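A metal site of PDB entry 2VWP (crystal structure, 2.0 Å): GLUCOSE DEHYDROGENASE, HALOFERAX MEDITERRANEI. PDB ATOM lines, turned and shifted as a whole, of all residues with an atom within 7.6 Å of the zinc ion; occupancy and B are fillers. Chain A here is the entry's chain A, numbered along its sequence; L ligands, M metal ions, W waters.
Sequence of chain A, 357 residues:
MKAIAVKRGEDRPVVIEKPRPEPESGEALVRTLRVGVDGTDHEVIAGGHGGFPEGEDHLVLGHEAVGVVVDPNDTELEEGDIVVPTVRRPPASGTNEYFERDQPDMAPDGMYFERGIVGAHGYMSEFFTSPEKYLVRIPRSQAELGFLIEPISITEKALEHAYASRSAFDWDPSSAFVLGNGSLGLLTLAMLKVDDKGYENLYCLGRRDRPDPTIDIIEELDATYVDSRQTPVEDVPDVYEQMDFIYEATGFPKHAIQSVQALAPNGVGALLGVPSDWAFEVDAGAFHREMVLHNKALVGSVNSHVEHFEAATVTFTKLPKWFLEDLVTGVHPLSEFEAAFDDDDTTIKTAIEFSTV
The nearest printed residue that does not touch the zinc ion is Asp 38 (4.2 Å).
ND1 of His 63 sits close to OG1 of Thr 40, 3.3 Å away. The side-chain carboxylate (OE1) of Glu 64 is in salt-bridge range of the side-chain amino group (NZ) of Lys 349, 2.6 Å away. The backbone carbonyl oxygen of Glu 150 is in hydrogen-bond range of the side-chain hydroxyl of Ser 153 (2.7 Å). O of Glu 64 sits at hydrogen-bond distance from N of Gly 36 (2.9 Å).
The zinc ion is bound by water W1 (2.2 Å), the side-chain carboxylate (OE1) of Glu 150 (2.2 Å), the side-chain carboxylate (OE2) of Glu 64 (2.3 Å) and a ring nitrogen (NE2) of His 63 (2.3 Å).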
ATOM      1  N   GLY A  36     -31.124 -14.029 -25.735  1.00  0.00           N
ATOM      2  CA  GLY A  36     -30.087 -14.949 -25.326  1.00  0.00           C
ATOM      3  C   GLY A  36     -28.853 -14.790 -26.202  1.00  0.00           C
ATOM      4  O   GLY A  36     -28.931 -14.400 -27.364  1.00  0.00           O
ATOM      5  N   VAL A  37     -27.702 -15.096 -25.606  1.00  0.00           N
ATOM      6  CA  VAL A  37     -26.451 -15.189 -26.319  1.00  0.00           C
ATOM      7  C   VAL A  37     -26.155 -16.653 -26.577  1.00  0.00           C
ATOM      8  O   VAL A  37     -26.343 -17.510 -25.711  1.00  0.00           O
ATOM      9  CB  VAL A  37     -25.286 -14.561 -25.511  1.00  0.00           C
ATOM     10  CG1 VAL A  37     -23.941 -14.856 -26.199  1.00  0.00           C
ATOM     11  CG2 VAL A  37     -25.489 -13.065 -25.341  1.00  0.00           C
ATOM     12  N   ASP A  38     -25.641 -16.910 -27.768  1.00  0.00           N
ATOM     13  CA  ASP A  38     -25.346 -18.232 -28.248  1.00  0.00           C
ATOM     14  C   ASP A  38     -23.934 -18.259 -28.838  1.00  0.00           C
ATOM     15  O   ASP A  38     -23.363 -17.200 -29.118  1.00  0.00           O
ATOM     16  CB  ASP A  38     -26.349 -18.557 -29.353  1.00  0.00           C
ATOM     17  CG  ASP A  38     -26.207 -19.931 -29.852  1.00  0.00           C
ATOM     18  OD1 ASP A  38     -26.461 -20.858 -29.068  1.00  0.00           O
ATOM     19  OD2 ASP A  38     -25.821 -20.103 -31.022  1.00  0.00           O
ATOM     20  N   GLY A  39     -23.383 -19.462 -29.036  1.00  0.00           N
ATOM     21  CA  GLY A  39     -22.146 -19.692 -29.789  1.00  0.00           C
ATOM     22  C   GLY A  39     -22.072 -18.992 -31.133  1.00  0.00           C
ATOM     23  O   GLY A  39     -21.023 -18.464 -31.489  1.00  0.00           O
ATOM     24  N   THR A  40     -23.185 -18.971 -31.879  1.00  0.00           N
ATOM     25  CA  THR A  40     -23.207 -18.277 -33.179  1.00  0.00           C
ATOM     26  C   THR A  40     -22.923 -16.793 -33.053  1.00  0.00           C
ATOM     27  O   THR A  40     -22.347 -16.204 -33.967  1.00  0.00           O
ATOM     28  CB  THR A  40     -24.536 -18.460 -33.992  1.00  0.00           C
ATOM     29  OG1 THR A  40     -25.572 -17.665 -33.412  1.00  0.00           O
ATOM     30  CG2 THR A  40     -24.956 -19.921 -34.057  1.00  0.00           C
ATOM     31  N   ASP A  41     -23.347 -16.186 -31.949  1.00  0.00           N
ATOM     32  CA  ASP A  41     -23.060 -14.779 -31.690  1.00  0.00           C
ATOM     33  C   ASP A  41     -21.566 -14.602 -31.489  1.00  0.00           C
ATOM     34  O   ASP A  41     -20.985 -13.648 -31.999  1.00  0.00           O
ATOM     35  CB  ASP A  41     -23.825 -14.254 -30.479  1.00  0.00           C
ATOM     36  CG  ASP A  41     -25.321 -14.283 -30.696  1.00  0.00           C
ATOM     37  OD1 ASP A  41     -25.800 -13.542 -31.601  1.00  0.00           O
ATOM     38  OD2 ASP A  41     -26.004 -15.049 -29.982  1.00  0.00           O
ATOM     39  N   HIS A  63     -30.264 -14.155 -31.917  1.00  0.00           N
ATOM     40  CA  HIS A  63     -31.370 -14.819 -32.629  1.00  0.00           C
ATOM     41  C   HIS A  63     -32.385 -15.511 -31.697  1.00  0.00           C
ATOM     42  O   HIS A  63     -33.340 -16.153 -32.176  1.00  0.00           O
ATOM     43  CB  HIS A  63     -30.807 -15.803 -33.666  1.00  0.00           C
ATOM     44  CG  HIS A  63     -30.112 -16.985 -33.053  1.00  0.00           C
ATOM     45  ND1 HIS A  63     -28.761 -16.989 -32.785  1.00  0.00           N
ATOM     46  CD2 HIS A  63     -30.581 -18.192 -32.659  1.00  0.00           C
ATOM     47  CE1 HIS A  63     -28.424 -18.150 -32.240  1.00  0.00           C
ATOM     48  NE2 HIS A  63     -29.508 -18.902 -32.173  1.00  0.00           N
ATOM     49  N   GLU A  64     -32.165 -15.395 -30.380  1.00  0.00           N
ATOM     50  CA  GLU A  64     -32.991 -16.086 -29.359  1.00  0.00           C
ATOM     51  C   GLU A  64     -33.747 -15.041 -28.557  1.00  0.00           C
ATOM     52  O   GLU A  64     -33.292 -14.591 -27.516  1.00  0.00           O
ATOM     53  CB  GLU A  64     -32.087 -16.906 -28.417  1.00  0.00           C
ATOM     54  CG  GLU A  64     -31.146 -17.854 -29.164  1.00  0.00           C
ATOM     55  CD  GLU A  64     -30.266 -18.662 -28.263  1.00  0.00           C
ATOM     56  OE1 GLU A  64     -29.944 -18.209 -27.139  1.00  0.00           O
ATOM     57  OE2 GLU A  64     -29.848 -19.761 -28.704  1.00  0.00           O
ATOM     58  N   VAL A  87     -36.251 -17.734 -36.643  1.00  0.00           N
ATOM     59  CA  VAL A  87     -34.979 -17.159 -37.086  1.00  0.00           C
ATOM     60  C   VAL A  87     -34.919 -16.944 -38.606  1.00  0.00           C
ATOM     61  O   VAL A  87     -34.362 -15.930 -39.046  1.00  0.00           O
ATOM     62  CB  VAL A  87     -33.767 -18.002 -36.612  1.00  0.00           C
ATOM     63  CG1 VAL A  87     -32.418 -17.315 -36.976  1.00  0.00           C
ATOM     64  CG2 VAL A  87     -33.867 -18.239 -35.095  1.00  0.00           C
ATOM     65  N   ILE A 117     -27.600 -13.918 -37.787  1.00  0.00           N
ATOM     66  CA  ILE A 117     -26.597 -14.923 -38.187  1.00  0.00           C
ATOM     67  C   ILE A 117     -26.046 -14.725 -39.609  1.00  0.00           C
ATOM     68  O   ILE A 117     -24.827 -14.631 -39.790  1.00  0.00           O
ATOM     69  CB  ILE A 117     -27.094 -16.390 -37.996  1.00  0.00           C
ATOM     70  CG1 ILE A 117     -27.686 -16.603 -36.584  1.00  0.00           C
ATOM     71  CG2 ILE A 117     -25.924 -17.361 -38.328  1.00  0.00           C
ATOM     72  CD1 ILE A 117     -28.258 -17.982 -36.334  1.00  0.00           C
ATOM     73  N   PHE A 147     -36.285 -16.306 -23.894  1.00  0.00           N
ATOM     74  CA  PHE A 147     -35.141 -16.439 -24.795  1.00  0.00           C
ATOM     75  C   PHE A 147     -34.711 -17.921 -24.893  1.00  0.00           C
ATOM     76  O   PHE A 147     -33.926 -18.270 -25.776  1.00  0.00           O
ATOM     77  CB  PHE A 147     -33.971 -15.507 -24.346  1.00  0.00           C
ATOM     78  CG  PHE A 147     -33.470 -15.800 -22.952  1.00  0.00           C
ATOM     79  CD1 PHE A 147     -32.559 -16.825 -22.717  1.00  0.00           C
ATOM     80  CD2 PHE A 147     -33.916 -15.046 -21.861  1.00  0.00           C
ATOM     81  CE1 PHE A 147     -32.094 -17.095 -21.391  1.00  0.00           C
ATOM     82  CE2 PHE A 147     -33.474 -15.303 -20.563  1.00  0.00           C
ATOM     83  CZ  PHE A 147     -32.553 -16.328 -20.329  1.00  0.00           C
ATOM     84  N   ILE A 149     -36.826 -20.392 -25.545  1.00  0.00           N
ATOM     85  CA  ILE A 149     -37.764 -21.119 -26.397  1.00  0.00           C
ATOM     86  C   ILE A 149     -37.109 -21.516 -27.713  1.00  0.00           C
ATOM     87  O   ILE A 149     -37.253 -22.656 -28.150  1.00  0.00           O
ATOM     88  CB  ILE A 149     -39.075 -20.340 -26.638  1.00  0.00           C
ATOM     89  CG1 ILE A 149     -39.890 -20.264 -25.337  1.00  0.00           C
ATOM     90  CG2 ILE A 149     -39.873 -20.958 -27.822  1.00  0.00           C
ATOM     91  CD1 ILE A 149     -40.244 -21.645 -24.680  1.00  0.00           C
ATOM     92  N   GLU A 150     -36.388 -20.582 -28.334  1.00  0.00           N
ATOM     93  CA  GLU A 150     -35.665 -20.924 -29.567  1.00  0.00           C
ATOM     94  C   GLU A 150     -34.702 -22.124 -29.426  1.00  0.00           C
ATOM     95  O   GLU A 150     -34.781 -23.051 -30.230  1.00  0.00           O
ATOM     96  CB  GLU A 150     -34.987 -19.680 -30.203  1.00  0.00           C
ATOM     97  CG  GLU A 150     -34.518 -19.868 -31.664  1.00  0.00           C
ATOM     98  CD  GLU A 150     -33.168 -20.547 -31.767  1.00  0.00           C
ATOM     99  OE1 GLU A 150     -32.450 -20.591 -30.735  1.00  0.00           O
ATOM    100  OE2 GLU A 150     -32.801 -21.046 -32.838  1.00  0.00           O
ATOM    101  N   PRO A 151     -33.740 -22.098 -28.462  1.00  0.00           N
ATOM    102  CA  PRO A 151     -32.883 -23.310 -28.389  1.00  0.00           C
ATOM    103  C   PRO A 151     -33.627 -24.607 -28.036  1.00  0.00           C
ATOM    104  O   PRO A 151     -33.267 -25.661 -28.552  1.00  0.00           O
ATOM    105  CB  PRO A 151     -31.805 -22.966 -27.342  1.00  0.00           C
ATOM    106  CG  PRO A 151     -32.297 -21.780 -26.615  1.00  0.00           C
ATOM    107  CD  PRO A 151     -33.261 -21.033 -27.561  1.00  0.00           C
ATOM    108  N   ILE A 152     -34.643 -24.539 -27.179  1.00  0.00           N
ATOM    109  CA  ILE A 152     -35.488 -25.731 -26.936  1.00  0.00           C
ATOM    110  C   ILE A 152     -36.068 -26.248 -28.253  1.00  0.00           C
ATOM    111  O   ILE A 152     -36.082 -27.444 -28.471  1.00  0.00           O
ATOM    112  CB  ILE A 152     -36.586 -25.473 -25.863  1.00  0.00           C
ATOM    113  CG1 ILE A 152     -35.910 -25.257 -24.501  1.00  0.00           C
ATOM    114  CG2 ILE A 152     -37.566 -26.668 -25.772  1.00  0.00           C
ATOM    115  CD1 ILE A 152     -36.780 -24.622 -23.436  1.00  0.00           C
ATOM    116  N   SER A 153     -36.524 -25.334 -29.114  1.00  0.00           N
ATOM    117  CA  SER A 153     -37.151 -25.672 -30.387  1.00  0.00           C
ATOM    118  C   SER A 153     -36.191 -26.385 -31.356  1.00  0.00           C
ATOM    119  O   SER A 153     -36.620 -27.223 -32.141  1.00  0.00           O
ATOM    120  CB  SER A 153     -37.792 -24.416 -31.060  1.00  0.00           C
ATOM    121  OG  SER A 153     -36.852 -23.665 -31.824  1.00  0.00           O
ATOM    122  N   ILE A 154     -34.901 -26.063 -31.288  1.00  0.00           N
ATOM    123  CA  ILE A 154     -33.885 -26.743 -32.072  1.00  0.00           C
ATOM    124  C   ILE A 154     -33.901 -28.263 -31.786  1.00  0.00           C
ATOM    125  O   ILE A 154     -33.871 -29.105 -32.712  1.00  0.00           O
ATOM    126  CB  ILE A 154     -32.465 -26.178 -31.774  1.00  0.00           C
ATOM    127  CG1 ILE A 154     -32.343 -24.709 -32.223  1.00  0.00           C
ATOM    128  CG2 ILE A 154     -31.380 -27.081 -32.373  1.00  0.00           C
ATOM    129  CD1 ILE A 154     -32.386 -24.476 -33.769  1.00  0.00           C
ATOM    130  N   LEU A 184     -27.142 -26.010 -25.185  1.00  0.00           N
ATOM    131  CA  LEU A 184     -27.974 -26.917 -25.993  1.00  0.00           C
ATOM    132  C   LEU A 184     -27.969 -28.352 -25.472  1.00  0.00           C
ATOM    133  O   LEU A 184     -29.028 -28.987 -25.344  1.00  0.00           O
ATOM    134  CB  LEU A 184     -27.608 -26.903 -27.478  1.00  0.00           C
ATOM    135  CG  LEU A 184     -28.584 -27.649 -28.411  1.00  0.00           C
ATOM    136  CD1 LEU A 184     -29.956 -26.944 -28.442  1.00  0.00           C
ATOM    137  CD2 LEU A 184     -28.010 -27.792 -29.828  1.00  0.00           C
ATOM    138  N   LYS A 349     -25.682 -20.242 -19.872  1.00  0.00           N
ATOM    139  CA  LYS A 349     -26.551 -19.455 -20.765  1.00  0.00           C
ATOM    140  C   LYS A 349     -26.686 -18.054 -20.177  1.00  0.00           C
ATOM    141  O   LYS A 349     -27.000 -17.887 -18.991  1.00  0.00           O
ATOM    142  CB  LYS A 349     -27.921 -20.155 -20.960  1.00  0.00           C
ATOM    143  CG  LYS A 349     -29.032 -19.322 -21.642  1.00  0.00           C
ATOM    144  CD  LYS A 349     -28.661 -18.813 -23.037  1.00  0.00           C
ATOM    145  CE  LYS A 349     -28.568 -19.922 -24.059  1.00  0.00           C
ATOM    146  NZ  LYS A 349     -28.336 -19.414 -25.442  1.00  0.00           N
HETATM  147  P1  LIG L   1     -20.903 -25.332 -27.198  1.00  0.00           P
HETATM  148  O1  LIG L   1     -21.059 -24.354 -26.098  1.00  0.00           O
HETATM  149  O2  LIG L   1     -19.595 -25.191 -27.924  1.00  0.00           O
HETATM  150  O3  LIG L   1     -21.053 -26.822 -26.617  1.00  0.00           O
HETATM  151  C1  LIG L   1     -20.205 -27.832 -27.074  1.00  0.00           C
HETATM  152  C2  LIG L   1     -19.707 -28.560 -25.838  1.00  0.00           C
HETATM  153  O4  LIG L   1     -19.129 -29.757 -26.287  1.00  0.00           O
HETATM  154  C3  LIG L   1     -18.637 -27.759 -25.081  1.00  0.00           C
HETATM  155  O5  LIG L   1     -19.058 -27.535 -23.740  1.00  0.00           O
HETATM  156  C4  LIG L   1     -17.388 -28.617 -25.199  1.00  0.00           C
HETATM  157  O6  LIG L   1     -16.694 -28.764 -23.988  1.00  0.00           O
HETATM  158  C5  LIG L   1     -17.946 -29.991 -25.563  1.00  0.00           C
HETATM  159  N1  LIG L   1     -17.001 -30.772 -26.363  1.00  0.00           N
HETATM  160  C6  LIG L   1     -16.410 -30.463 -27.567  1.00  0.00           C
HETATM  161  N2  LIG L   1     -15.602 -31.508 -27.904  1.00  0.00           N
HETATM  162  C7  LIG L   1     -15.678 -32.449 -26.922  1.00  0.00           C
HETATM  163  C8  LIG L   1     -15.071 -33.692 -26.732  1.00  0.00           C
HETATM  164  N3  LIG L   1     -14.109 -34.127 -27.547  1.00  0.00           N
HETATM  165  N4  LIG L   1     -15.384 -34.413 -25.585  1.00  0.00           N
HETATM  166  C9  LIG L   1     -16.264 -33.934 -24.644  1.00  0.00           C
HETATM  167  N5  LIG L   1     -16.851 -32.720 -24.835  1.00  0.00           N
HETATM  168  C10 LIG L   1     -16.565 -31.989 -25.945  1.00  0.00           C
HETATM  169  O7  LIG L   1     -22.172 -25.145 -28.210  1.00  0.00           O
HETATM  170  P2  LIG L   1     -23.764 -25.437 -27.955  1.00  0.00           P
HETATM  171  O8  LIG L   1     -24.023 -26.446 -26.895  1.00  0.00           O
HETATM  172  O9  LIG L   1     -24.515 -24.157 -27.857  1.00  0.00           O
HETATM  173  O10 LIG L   1     -24.023 -26.121 -29.397  1.00  0.00           O
HETATM  174  C11 LIG L   1     -23.468 -27.407 -29.669  1.00  0.00           C
HETATM  175  C12 LIG L   1     -23.121 -27.647 -31.151  1.00  0.00           C
HETATM  176  O11 LIG L   1     -24.325 -27.649 -31.909  1.00  0.00           O
HETATM  177  C13 LIG L   1     -22.181 -26.620 -31.790  1.00  0.00           C
HETATM  178  O12 LIG L   1     -21.330 -27.241 -32.734  1.00  0.00           O
HETATM  179  C14 LIG L   1     -23.118 -25.704 -32.536  1.00  0.00           C
HETATM  180  O13 LIG L   1     -22.525 -25.172 -33.703  1.00  0.00           O
HETATM  181  C15 LIG L   1     -24.252 -26.653 -32.908  1.00  0.00           C
HETATM  182  N6  LIG L   1     -25.560 -26.000 -33.006  1.00  0.00           N
HETATM  183  C16 LIG L   1     -26.371 -26.465 -33.999  1.00  0.00           C
HETATM  184  C17 LIG L   1     -27.700 -26.083 -34.121  1.00  0.00           C
HETATM  185  C18 LIG L   1     -28.514 -26.663 -35.257  1.00  0.00           C
HETATM  186  O14 LIG L   1     -29.758 -26.083 -35.534  1.00  0.00           O
HETATM  187  N7  LIG L   1     -28.052 -27.706 -35.975  1.00  0.00           N
HETATM  188  C19 LIG L   1     -28.309 -25.096 -33.144  1.00  0.00           C
HETATM  189  C20 LIG L   1     -27.320 -24.660 -32.087  1.00  0.00           C
HETATM  190  C21 LIG L   1     -26.000 -25.119 -32.059  1.00  0.00           C
HETATM  191  P3  LIG L   1     -15.541 -27.752 -23.507  1.00  0.00           P
HETATM  192  O15 LIG L   1     -16.103 -26.365 -23.320  1.00  0.00           O
HETATM  193  O16 LIG L   1     -14.475 -27.642 -24.586  1.00  0.00           O
HETATM  194  O17 LIG L   1     -15.058 -28.400 -22.225  1.00  0.00           O
HETATM  195 ZN    ZN M   1     -30.265 -20.583 -30.778  1.00  0.00          ZN
HETATM  196  O   HOH W   1     -29.656 -22.662 -30.942  1.00  0.00           O
